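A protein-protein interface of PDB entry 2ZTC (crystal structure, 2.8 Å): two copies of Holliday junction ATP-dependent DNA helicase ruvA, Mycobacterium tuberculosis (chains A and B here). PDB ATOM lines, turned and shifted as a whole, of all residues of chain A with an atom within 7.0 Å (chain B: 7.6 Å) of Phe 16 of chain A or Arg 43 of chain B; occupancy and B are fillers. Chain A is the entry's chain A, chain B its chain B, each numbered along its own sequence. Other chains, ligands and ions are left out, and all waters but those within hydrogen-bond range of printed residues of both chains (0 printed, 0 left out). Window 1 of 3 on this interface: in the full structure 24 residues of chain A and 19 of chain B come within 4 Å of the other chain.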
ATOM      1  N   SER A  14     -13.271 -25.982 -30.489  1.00  0.00           N
ATOM      2  CA  SER A  14     -11.923 -26.446 -30.805  1.00  0.00           C
ATOM      3  C   SER A  14     -10.820 -26.416 -29.746  1.00  0.00           C
ATOM      4  O   SER A  14      -9.896 -27.226 -29.797  1.00  0.00           O
ATOM      5  CB  SER A  14     -11.501 -25.586 -31.998  1.00  0.00           C
ATOM      6  N   GLU A  15     -10.903 -25.484 -28.803  1.00  0.00           N
ATOM      7  CA  GLU A  15      -9.743 -25.133 -27.977  1.00  0.00           C
ATOM      8  C   GLU A  15      -9.735 -25.661 -26.523  1.00  0.00           C
ATOM      9  O   GLU A  15     -10.658 -25.415 -25.730  1.00  0.00           O
ATOM     10  CB  GLU A  15      -9.533 -23.609 -28.011  1.00  0.00           C
ATOM     11  N   PHE A  16      -8.675 -26.399 -26.199  1.00  0.00           N
ATOM     12  CA  PHE A  16      -8.447 -26.939 -24.862  1.00  0.00           C
ATOM     13  C   PHE A  16      -7.145 -26.373 -24.338  1.00  0.00           C
ATOM     14  O   PHE A  16      -6.626 -25.384 -24.860  1.00  0.00           O
ATOM     15  CB  PHE A  16      -8.388 -28.471 -24.896  1.00  0.00           C
ATOM     16  N   MET A  17      -6.615 -27.001 -23.305  1.00  0.00           N
ATOM     17  CA  MET A  17      -5.484 -26.439 -22.589  1.00  0.00           C
ATOM     18  C   MET A  17      -4.275 -27.349 -22.607  1.00  0.00           C
ATOM     19  O   MET A  17      -3.174 -26.915 -22.942  1.00  0.00           O
ATOM     20  CB  MET A  17      -5.851 -26.205 -21.133  1.00  0.00           C
ATOM     21  CG  MET A  17      -4.694 -25.651 -20.308  1.00  0.00           C
ATOM     22  SD  MET A  17      -5.160 -25.328 -18.598  1.00  0.00           S
ATOM     23  CE  MET A  17      -6.731 -24.517 -18.831  1.00  0.00           C
ATOM     24  N   ILE A  18      -4.462 -28.612 -22.222  1.00  0.00           N
ATOM     25  CA  ILE A  18      -3.351 -29.565 -22.245  1.00  0.00           C
ATOM     26  C   ILE A  18      -3.285 -30.277 -23.571  1.00  0.00           C
ATOM     27  O   ILE A  18      -4.149 -31.071 -23.912  1.00  0.00           O
ATOM     28  CB  ILE A  18      -3.448 -30.595 -21.143  1.00  0.00           C
ATOM     29  CG1 ILE A  18      -3.637 -29.887 -19.803  1.00  0.00           C
ATOM     30  CG2 ILE A  18      -2.173 -31.442 -21.124  1.00  0.00           C
ATOM     31  CD1 ILE A  18      -3.222 -30.694 -18.669  1.00  0.00           C
ATOM     32  N   ALA A  19      -2.274 -29.934 -24.345  1.00  0.00           N
ATOM     33  CA  ALA A  19      -2.197 -30.387 -25.716  1.00  0.00           C
ATOM     34  C   ALA A  19      -1.137 -31.462 -25.881  1.00  0.00           C
ATOM     35  O   ALA A  19      -0.928 -31.958 -26.974  1.00  0.00           O
ATOM     36  CB  ALA A  19      -1.893 -29.229 -26.614  1.00  0.00           C
ATOM     37  N   SER A  20      -0.464 -31.819 -24.794  1.00  0.00           N
ATOM     38  CA  SER A  20       0.515 -32.902 -24.833  1.00  0.00           C
ATOM     39  C   SER A  20       1.058 -33.206 -23.455  1.00  0.00           C
ATOM     40  O   SER A  20       1.070 -32.335 -22.575  1.00  0.00           O
ATOM     41  CB  SER A  20       1.682 -32.534 -25.755  1.00  0.00           C
ATOM     42  OG  SER A  20       2.781 -31.972 -25.044  1.00  0.00           O
ATOM     43  N   THR A  64      -2.146 -34.845 -26.839  1.00  0.00           N
ATOM     44  CA  THR A  64      -3.379 -35.131 -26.139  1.00  0.00           C
ATOM     45  C   THR A  64      -4.472 -34.149 -26.503  1.00  0.00           C
ATOM     46  O   THR A  64      -4.215 -33.048 -26.991  1.00  0.00           O
ATOM     47  CB  THR A  64      -3.156 -35.039 -24.635  1.00  0.00           C
ATOM     48  OG1 THR A  64      -2.977 -33.666 -24.266  1.00  0.00           O
ATOM     49  CG2 THR A  64      -1.902 -35.792 -24.267  1.00  0.00           C
ATOM     50  N   ALA A  65      -5.700 -34.582 -26.276  1.00  0.00           N
ATOM     51  CA  ALA A  65      -6.846 -33.702 -26.324  1.00  0.00           C
ATOM     52  C   ALA A  65      -7.517 -33.799 -24.966  1.00  0.00           C
ATOM     53  O   ALA A  65      -7.635 -34.880 -24.392  1.00  0.00           O
ATOM     54  CB  ALA A  65      -7.790 -34.112 -27.411  1.00  0.00           C
ATOM     55  N   MET A  66      -7.930 -32.654 -24.445  1.00  0.00           N
ATOM     56  CA  MET A  66      -8.456 -32.579 -23.105  1.00  0.00           C
ATOM     57  C   MET A  66      -9.949 -32.326 -23.174  1.00  0.00           C
ATOM     58  O   MET A  66     -10.400 -31.455 -23.922  1.00  0.00           O
ATOM     59  CB  MET A  66      -7.743 -31.466 -22.338  1.00  0.00           C
ATOM     60  CG  MET A  66      -8.341 -31.149 -20.974  1.00  0.00           C
ATOM     61  SD  MET A  66      -7.226 -30.202 -19.896  1.00  0.00           S
ATOM     62  CE  MET A  66      -8.438 -29.531 -18.785  1.00  0.00           C
ATOM     63  N   ILE A  67     -10.718 -33.096 -22.414  1.00  0.00           N
ATOM     64  CA  ILE A  67     -12.154 -32.887 -22.371  1.00  0.00           C
ATOM     65  C   ILE A  67     -12.635 -32.657 -20.961  1.00  0.00           C
ATOM     66  O   ILE A  67     -12.479 -33.524 -20.091  1.00  0.00           O
ATOM     67  CB  ILE A  67     -12.923 -34.053 -22.959  1.00  0.00           C
ATOM     68  CG1 ILE A  67     -12.637 -34.146 -24.451  1.00  0.00           C
ATOM     69  CG2 ILE A  67     -14.411 -33.883 -22.709  1.00  0.00           C
ATOM     70  CD1 ILE A  67     -13.238 -35.367 -25.052  1.00  0.00           C
ATOM     71  N   ARG A  84      -4.516 -36.783 -33.260  1.00  0.00           N
ATOM     72  CA  ARG A  84      -5.259 -36.040 -32.252  1.00  0.00           C
ATOM     73  C   ARG A  84      -6.272 -35.096 -32.911  1.00  0.00           C
ATOM     74  O   ARG A  84      -7.436 -35.065 -32.535  1.00  0.00           O
ATOM     75  CB  ARG A  84      -4.296 -35.277 -31.353  1.00  0.00           C
ATOM     76  CG  ARG A  84      -4.904 -34.711 -30.089  1.00  0.00           C
ATOM     77  CD  ARG A  84      -5.480 -33.318 -30.323  1.00  0.00           C
ATOM     78  NE  ARG A  84      -4.601 -32.492 -31.144  1.00  0.00           N
ATOM     79  CZ  ARG A  84      -3.572 -31.801 -30.673  1.00  0.00           C
ATOM     80  NH1 ARG A  84      -3.292 -31.820 -29.373  1.00  0.00           N
ATOM     81  NH2 ARG A  84      -2.822 -31.089 -31.505  1.00  0.00           N
ATOM     82  N   LEU A  88     -10.542 -34.969 -32.560  1.00  0.00           N
ATOM     83  CA  LEU A  88     -11.432 -33.818 -32.386  1.00  0.00           C
ATOM     84  C   LEU A  88     -12.493 -33.772 -33.461  1.00  0.00           C
ATOM     85  O   LEU A  88     -13.676 -33.612 -33.163  1.00  0.00           O
ATOM     86  CB  LEU A  88     -10.657 -32.509 -32.418  1.00  0.00           C
ATOM     87  CG  LEU A  88      -9.930 -32.019 -31.157  1.00  0.00           C
ATOM     88  CD1 LEU A  88     -10.744 -32.347 -29.918  1.00  0.00           C
ATOM     89  CD2 LEU A  88      -8.541 -32.639 -31.077  1.00  0.00           C
ATOM     90  N   VAL B  21       3.079 -18.855 -18.792  1.00  0.00           N
ATOM     91  CA  VAL B  21       3.669 -20.167 -19.064  1.00  0.00           C
ATOM     92  C   VAL B  21       5.049 -20.017 -19.685  1.00  0.00           C
ATOM     93  O   VAL B  21       5.239 -19.239 -20.606  1.00  0.00           O
ATOM     94  CB  VAL B  21       2.774 -21.045 -19.995  1.00  0.00           C
ATOM     95  CG1 VAL B  21       3.207 -22.501 -19.942  1.00  0.00           C
ATOM     96  CG2 VAL B  21       1.309 -20.927 -19.604  1.00  0.00           C
ATOM     97  N   GLU B  27       5.417 -26.069 -30.949  1.00  0.00           N
ATOM     98  CA  GLU B  27       4.638 -25.883 -32.155  1.00  0.00           C
ATOM     99  C   GLU B  27       4.227 -24.418 -32.196  1.00  0.00           C
ATOM    100  O   GLU B  27       3.754 -23.878 -31.199  1.00  0.00           O
ATOM    101  CB  GLU B  27       3.400 -26.779 -32.103  1.00  0.00           C
ATOM    102  CG  GLU B  27       2.467 -26.702 -33.310  1.00  0.00           C
ATOM    103  CD  GLU B  27       1.123 -27.373 -33.048  1.00  0.00           C
ATOM    104  OE1 GLU B  27       1.003 -28.101 -32.040  1.00  0.00           O
ATOM    105  OE2 GLU B  27       0.186 -27.167 -33.847  1.00  0.00           O
ATOM    106  N   ALA B  29       1.639 -22.189 -34.392  1.00  0.00           N
ATOM    107  CA  ALA B  29       0.625 -22.201 -35.440  1.00  0.00           C
ATOM    108  C   ALA B  29       0.225 -20.780 -35.800  1.00  0.00           C
ATOM    109  O   ALA B  29       0.941 -19.833 -35.506  1.00  0.00           O
ATOM    110  CB  ALA B  29      -0.586 -23.013 -35.026  1.00  0.00           C
ATOM    111  N   ASP B  31      -2.792 -19.482 -34.856  1.00  0.00           N
ATOM    112  CA  ASP B  31      -3.759 -18.976 -33.898  1.00  0.00           C
ATOM    113  C   ASP B  31      -3.439 -19.441 -32.487  1.00  0.00           C
ATOM    114  O   ASP B  31      -4.206 -19.190 -31.542  1.00  0.00           O
ATOM    115  CB  ASP B  31      -5.167 -19.431 -34.262  1.00  0.00           C
ATOM    116  CG  ASP B  31      -5.350 -20.922 -34.091  1.00  0.00           C
ATOM    117  OD1 ASP B  31      -4.342 -21.652 -34.170  1.00  0.00           O
ATOM    118  OD2 ASP B  31      -6.496 -21.368 -33.874  1.00  0.00           O
ATOM    119  N   HIS B  32      -2.312 -20.124 -32.343  1.00  0.00           N
ATOM    120  CA  HIS B  32      -1.899 -20.564 -31.026  1.00  0.00           C
ATOM    121  C   HIS B  32      -0.488 -21.088 -31.036  1.00  0.00           C
ATOM    122  O   HIS B  32       0.153 -21.161 -32.073  1.00  0.00           O
ATOM    123  CB  HIS B  32      -2.816 -21.667 -30.540  1.00  0.00           C
ATOM    124  CG  HIS B  32      -2.662 -22.940 -31.304  1.00  0.00           C
ATOM    125  ND1 HIS B  32      -3.545 -23.335 -32.287  1.00  0.00           N
ATOM    126  CD2 HIS B  32      -1.738 -23.928 -31.214  1.00  0.00           C
ATOM    127  CE1 HIS B  32      -3.163 -24.500 -32.777  1.00  0.00           C
ATOM    128  NE2 HIS B  32      -2.075 -24.877 -32.147  1.00  0.00           N
ATOM    129  N   VAL B  33      -0.027 -21.478 -29.857  1.00  0.00           N
ATOM    130  CA  VAL B  33       1.313 -21.995 -29.662  1.00  0.00           C
ATOM    131  C   VAL B  33       1.250 -23.098 -28.616  1.00  0.00           C
ATOM    132  O   VAL B  33       0.281 -23.210 -27.876  1.00  0.00           O
ATOM    133  CB  VAL B  33       2.264 -20.892 -29.153  1.00  0.00           C
ATOM    134  CG1 VAL B  33       1.759 -20.345 -27.851  1.00  0.00           C
ATOM    135  CG2 VAL B  33       3.676 -21.429 -28.969  1.00  0.00           C
ATOM    136  N   VAL B  34       2.285 -23.912 -28.549  1.00  0.00           N
ATOM    137  CA  VAL B  34       2.341 -24.940 -27.542  1.00  0.00           C
ATOM    138  C   VAL B  34       3.643 -24.821 -26.768  1.00  0.00           C
ATOM    139  O   VAL B  34       4.705 -25.245 -27.244  1.00  0.00           O
ATOM    140  CB  VAL B  34       2.231 -26.353 -28.163  1.00  0.00           C
ATOM    141  CG1 VAL B  34       2.359 -27.401 -27.070  1.00  0.00           C
ATOM    142  CG2 VAL B  34       0.907 -26.507 -28.899  1.00  0.00           C
ATOM    143  N   ILE B  35       3.550 -24.236 -25.576  1.00  0.00           N
ATOM    144  CA  ILE B  35       4.682 -24.147 -24.668  1.00  0.00           C
ATOM    145  C   ILE B  35       4.686 -25.349 -23.731  1.00  0.00           C
ATOM    146  O   ILE B  35       3.675 -25.641 -23.080  1.00  0.00           O
ATOM    147  CB  ILE B  35       4.601 -22.885 -23.796  1.00  0.00           C
ATOM    148  CG1 ILE B  35       4.193 -21.679 -24.622  1.00  0.00           C
ATOM    149  CG2 ILE B  35       5.942 -22.613 -23.112  1.00  0.00           C
ATOM    150  CD1 ILE B  35       3.849 -20.496 -23.771  1.00  0.00           C
ATOM    151  N   GLU B  36       5.828 -26.030 -23.660  1.00  0.00           N
ATOM    152  CA  GLU B  36       5.986 -27.164 -22.759  1.00  0.00           C
ATOM    153  C   GLU B  36       6.648 -26.777 -21.435  1.00  0.00           C
ATOM    154  O   GLU B  36       7.866 -26.624 -21.350  1.00  0.00           O
ATOM    155  CB  GLU B  36       6.754 -28.312 -23.422  1.00  0.00           C
ATOM    156  CG  GLU B  36       7.153 -29.406 -22.440  1.00  0.00           C
ATOM    157  CD  GLU B  36       7.704 -30.633 -23.117  1.00  0.00           C
ATOM    158  OE1 GLU B  36       6.906 -31.460 -23.595  1.00  0.00           O
ATOM    159  OE2 GLU B  36       8.938 -30.783 -23.157  1.00  0.00           O
ATOM    160  N   VAL B  40       4.370 -30.871 -19.403  1.00  0.00           N
ATOM    161  CA  VAL B  40       3.076 -30.557 -20.007  1.00  0.00           C
ATOM    162  C   VAL B  40       3.155 -29.576 -21.156  1.00  0.00           C
ATOM    163  O   VAL B  40       3.804 -28.549 -21.057  1.00  0.00           O
ATOM    164  CB  VAL B  40       2.125 -29.983 -18.972  1.00  0.00           C
ATOM    165  CG1 VAL B  40       0.747 -29.752 -19.588  1.00  0.00           C
ATOM    166  CG2 VAL B  40       2.026 -30.937 -17.823  1.00  0.00           C
ATOM    167  N   GLY B  41       2.483 -29.887 -22.247  1.00  0.00           N
ATOM    168  CA  GLY B  41       2.396 -28.941 -23.334  1.00  0.00           C
ATOM    169  C   GLY B  41       1.098 -28.183 -23.219  1.00  0.00           C
ATOM    170  O   GLY B  41       0.025 -28.697 -23.518  1.00  0.00           O
ATOM    171  N   TYR B  42       1.202 -26.955 -22.751  1.00  0.00           N
ATOM    172  CA  TYR B  42       0.051 -26.097 -22.640  1.00  0.00           C
ATOM    173  C   TYR B  42      -0.212 -25.462 -23.991  1.00  0.00           C
ATOM    174  O   TYR B  42       0.712 -24.973 -24.645  1.00  0.00           O
ATOM    175  CB  TYR B  42       0.293 -25.019 -21.559  1.00  0.00           C
ATOM    176  CG  TYR B  42       0.415 -25.592 -20.155  1.00  0.00           C
ATOM    177  CD1 TYR B  42       1.628 -26.083 -19.689  1.00  0.00           C
ATOM    178  CD2 TYR B  42      -0.684 -25.675 -19.314  1.00  0.00           C
ATOM    179  CE1 TYR B  42       1.743 -26.624 -18.410  1.00  0.00           C
ATOM    180  CE2 TYR B  42      -0.581 -26.205 -18.032  1.00  0.00           C
ATOM    181  CZ  TYR B  42       0.633 -26.682 -17.583  1.00  0.00           C
ATOM    182  OH  TYR B  42       0.736 -27.216 -16.308  1.00  0.00           O
ATOM    183  N   ARG B  43      -1.470 -25.483 -24.417  1.00  0.00           N
ATOM    184  CA  ARG B  43      -1.879 -24.713 -25.593  1.00  0.00           C
ATOM    185  C   ARG B  43      -2.435 -23.369 -25.197  1.00  0.00           C
ATOM    186  O   ARG B  43      -3.512 -23.279 -24.562  1.00  0.00           O
ATOM    187  CB  ARG B  43      -2.963 -25.420 -26.397  1.00  0.00           C
ATOM    188  CG  ARG B  43      -3.630 -24.538 -27.438  1.00  0.00           C
ATOM    189  CD  ARG B  43      -4.866 -25.195 -28.014  1.00  0.00           C
ATOM    190  NE  ARG B  43      -4.962 -25.068 -29.470  1.00  0.00           N
ATOM    191  CZ  ARG B  43      -5.869 -24.331 -30.096  1.00  0.00           C
ATOM    192  NH1 ARG B  43      -6.768 -23.639 -29.413  1.00  0.00           N
ATOM    193  NH2 ARG B  43      -5.885 -24.297 -31.411  1.00  0.00           N
ATOM    194  N   VAL B  44      -1.719 -22.329 -25.610  1.00  0.00           N
ATOM    195  CA  VAL B  44      -2.184 -20.972 -25.429  1.00  0.00           C
ATOM    196  C   VAL B  44      -2.452 -20.336 -26.776  1.00  0.00           C
ATOM    197  O   VAL B  44      -1.610 -20.362 -27.659  1.00  0.00           O
ATOM    198  CB  VAL B  44      -1.190 -20.149 -24.587  1.00  0.00           C
ATOM    199  CG1 VAL B  44      -1.094 -20.720 -23.188  1.00  0.00           C
ATOM    200  CG2 VAL B  44       0.150 -20.102 -25.257  1.00  0.00           C
ATOM    201  N   ASN B  45      -3.649 -19.794 -26.931  1.00  0.00           N
ATOM    202  CA  ASN B  45      -4.004 -19.073 -28.135  1.00  0.00           C
ATOM    203  C   ASN B  45      -3.411 -17.666 -28.152  1.00  0.00           C
ATOM    204  O   ASN B  45      -3.114 -17.112 -27.104  1.00  0.00           O
ATOM    205  CB  ASN B  45      -5.514 -19.043 -28.243  1.00  0.00           C
ATOM    206  CG  ASN B  45      -6.094 -20.407 -28.083  1.00  0.00           C
ATOM    207  OD1 ASN B  45      -5.526 -21.381 -28.570  1.00  0.00           O
ATOM    208  ND2 ASN B  45      -7.209 -20.509 -27.381  1.00  0.00           N
ATOM    209  N   ALA B  46      -3.232 -17.090 -29.335  1.00  0.00           N
ATOM    210  CA  ALA B  46      -2.465 -15.864 -29.440  1.00  0.00           C
ATOM    211  C   ALA B  46      -2.651 -15.188 -30.802  1.00  0.00           C
ATOM    212  O   ALA B  46      -3.034 -15.834 -31.784  1.00  0.00           O
ATOM    213  CB  ALA B  46      -0.990 -16.162 -29.173  1.00  0.00           C
ATOM    214  N   SER B  72     -15.215 -26.002 -20.647  1.00  0.00           N
ATOM    215  CA  SER B  72     -14.036 -25.454 -21.302  1.00  0.00           C
ATOM    216  C   SER B  72     -12.954 -25.045 -20.304  1.00  0.00           C
ATOM    217  O   SER B  72     -13.252 -24.636 -19.186  1.00  0.00           O
ATOM    218  CB  SER B  72     -14.449 -24.228 -22.118  1.00  0.00           C
ATOM    219  OG  SER B  72     -14.770 -23.143 -21.260  1.00  0.00           O
ATOM    220  N   MET B  73     -11.695 -25.148 -20.711  1.00  0.00           N
ATOM    221  CA  MET B  73     -10.606 -24.602 -19.914  1.00  0.00           C
ATOM    222  C   MET B  73      -9.486 -24.126 -20.842  1.00  0.00           C
ATOM    223  O   MET B  73      -8.642 -24.918 -21.255  1.00  0.00           O
ATOM    224  CB  MET B  73     -10.108 -25.649 -18.917  1.00  0.00           C
ATOM    225  CG  MET B  73      -9.423 -25.074 -17.694  1.00  0.00           C
ATOM    226  SD  MET B  73      -9.276 -26.284 -16.385  1.00  0.00           S
ATOM    227  CE  MET B  73     -11.006 -26.434 -15.926  1.00  0.00           C
ATOM    228  N   THR B  74      -9.487 -22.834 -21.174  1.00  0.00           N
ATOM    229  CA  THR B  74      -8.581 -22.303 -22.213  1.00  0.00           C
ATOM    230  C   THR B  74      -7.584 -21.228 -21.764  1.00  0.00           C
ATOM    231  O   THR B  74      -7.862 -20.433 -20.870  1.00  0.00           O
ATOM    232  CB  THR B  74      -9.369 -21.657 -23.351  1.00  0.00           C
ATOM    233  OG1 THR B  74     -10.532 -22.436 -23.640  1.00  0.00           O
ATOM    234  CG2 THR B  74      -8.503 -21.540 -24.589  1.00  0.00           C
ATOM    235  N   LEU B  75      -6.434 -21.194 -22.416  1.00  0.00           N
ATOM    236  CA  LEU B  75      -5.439 -20.159 -22.164  1.00  0.00           C
ATOM    237  C   LEU B  75      -5.284 -19.173 -23.324  1.00  0.00           C
ATOM    238  O   LEU B  75      -5.214 -19.560 -24.486  1.00  0.00           O
ATOM    239  CB  LEU B  75      -4.070 -20.787 -21.927  1.00  0.00           C
ATOM    240  CG  LEU B  75      -3.872 -21.542 -20.636  1.00  0.00           C
ATOM    241  CD1 LEU B  75      -2.374 -21.680 -20.418  1.00  0.00           C
ATOM    242  CD2 LEU B  75      -4.509 -20.758 -19.516  1.00  0.00           C
ATOM    243  N   TYR B  76      -5.179 -17.892 -22.998  1.00  0.00           N
ATOM    244  CA  TYR B  76      -4.806 -16.895 -23.990  1.00  0.00           C
ATOM    245  C   TYR B  76      -3.528 -16.233 -23.529  1.00  0.00           C
ATOM    246  O   TYR B  76      -3.427 -15.804 -22.386  1.00  0.00           O
ATOM    247  CB  TYR B  76      -5.919 -15.879 -24.152  1.00  0.00           C
ATOM    248  CG  TYR B  76      -7.207 -16.543 -24.557  1.00  0.00           C
ATOM    249  CD1 TYR B  76      -8.036 -17.107 -23.609  1.00  0.00           C
ATOM    250  CD2 TYR B  76      -7.575 -16.633 -25.881  1.00  0.00           C
ATOM    251  CE1 TYR B  76      -9.208 -17.723 -23.961  1.00  0.00           C
ATOM    252  CE2 TYR B  76      -8.752 -17.248 -26.248  1.00  0.00           C
ATOM    253  CZ  TYR B  76      -9.567 -17.792 -25.277  1.00  0.00           C
ATOM    254  OH  TYR B  76     -10.746 -18.427 -25.608  1.00  0.00           O
ATOM    255  N   GLY B  77      -2.547 -16.194 -24.420  1.00  0.00           N
ATOM    256  CA  GLY B  77      -1.233 -15.636 -24.148  1.00  0.00           C
ATOM    257  C   GLY B  77      -0.921 -14.331 -24.860  1.00  0.00           C
ATOM    258  O   GLY B  77      -1.548 -13.982 -25.856  1.00  0.00           O
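The backbone NH (N) of Arg 43 of chain B lies within hydrogen-bond range of the backbone carbonyl oxygen (O) of Met 17 of chain A (2.7 Å). The backbone carbonyl oxygen of Gly 41 of chain B lies within hydrogen-bond range of the backbone NH of Ala 19 of chain A (2.7 Å). The backbone carbonyl oxygen (O) of Ser 20 of chain A lies within hydrogen-bond range of the backbone NH (N) of Gly 41 of chain B, at 2.8 Å.
The side-chain hydroxyl (OG1) of Thr 64 of chain A sits at hydrogen-bond distance from the backbone carbonyl oxygen (O) of Ile 18 of chain A. The backbone carbonyl oxygen (O) of Ala 19 of chain A is in hydrogen-bond range of the backbone NH (N) of Thr 64 of chain A (3.1 Å). The backbone carbonyl oxygen (O) of Ala 19 of chain A is in hydrogen-bond range of the guanidinium group (NH1) of Arg 84 of chain A (3.4 Å). N of Ser 20 of chain A lies within hydrogen-bond range of OG1 of Thr 64 of chain A, at 3.2 Å. ND1 of His 32 of chain B sits at hydrogen-bond distance from NH2 of Arg 43 of chain B, 2.7 Å away. The backbone NH (N) of Tyr 42 of chain B sits at hydrogen-bond distance from the backbone carbonyl oxygen (O) of Ile 35 of chain B (2.8 Å).
Among the printed residues, merely in contact across the chains: Met 17 of chain A with Met 73 of chain B (3.0 Å), Glu 15 of chain A with Arg 43 of chain B (3.1 Å), Met 17 of chain A with Tyr 42 of chain B (3.3 Å), Phe 16 of chain A with Arg 43 of chain B (3.6 Å), Glu 15 of chain A with Thr 74 of chain B (3.6 Å), Ile 18 of chain A with Gly 41 of chain B (3.7 Å), Met 17 of chain A with Gly 41 of chain B (3.7 Å), Ile 18 of chain A with Val 40 of chain B (3.7 Å), Ser 20 of chain A with Val 40 of chain B (3.7 Å), Phe 16 of chain A with Met 73 of chain B (3.7 Å), Glu 15 of chain A with Asn 45 of chain B (3.9 Å), Ala 19 of chain A with Arg 43 of chain B (3.96 Å) and Met 17 of chain A with Thr 74 of chain B (3.99 Å).
Glu 15 of chain A touches just these residues of chain B: Arg 43 (3.1 Å), Asn 45 (3.9 Å) and Thr 74 (3.6 Å). Of chain B, only Arg 43 (3.6 Å) and Met 73 (3.7 Å) come within 4 Å of Phe 16 of chain A. Of the printed residues of chain B, Met 17 of chain A touches Gly 41 (3.7 Å), Tyr 42 (3.3 Å), Arg 43 (2.7 Å), Met 73 (3.0 Å) and Thr 74 (3.99 Å). Leu 88 of chain A touches none of the printed residues of chain B. Printed residues of chain A within 4 Å of Val 40 of chain B: Ile 18 (3.7 Å) and Ser 20 (3.7 Å). Val 44 of chain B touches none of the printed residues of chain A. Printed residues of chain A within 4 Å of Asn 45 of chain B: Glu 15.
Of the 13 printed residues of chain A, 6 touch a printed residue of chain B. Of the 22 printed residues of chain B, 7 touch a printed residue of chain A. Hydrophobic or aromatic side chains of chain B that line the printed part of chain A: Val 40 and Met 73. Among the printed residues, 16 pairs touch across the chains. Among the printed residues, no Asp or Glu carboxylate lies within 4 Å of a Lys or Arg side-chain nitrogen of the other chain.
No position is printed for both chains. Of the 16 pairs that touch across the chains among the printed residues, none has its exchanged pair printed and touching as well.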
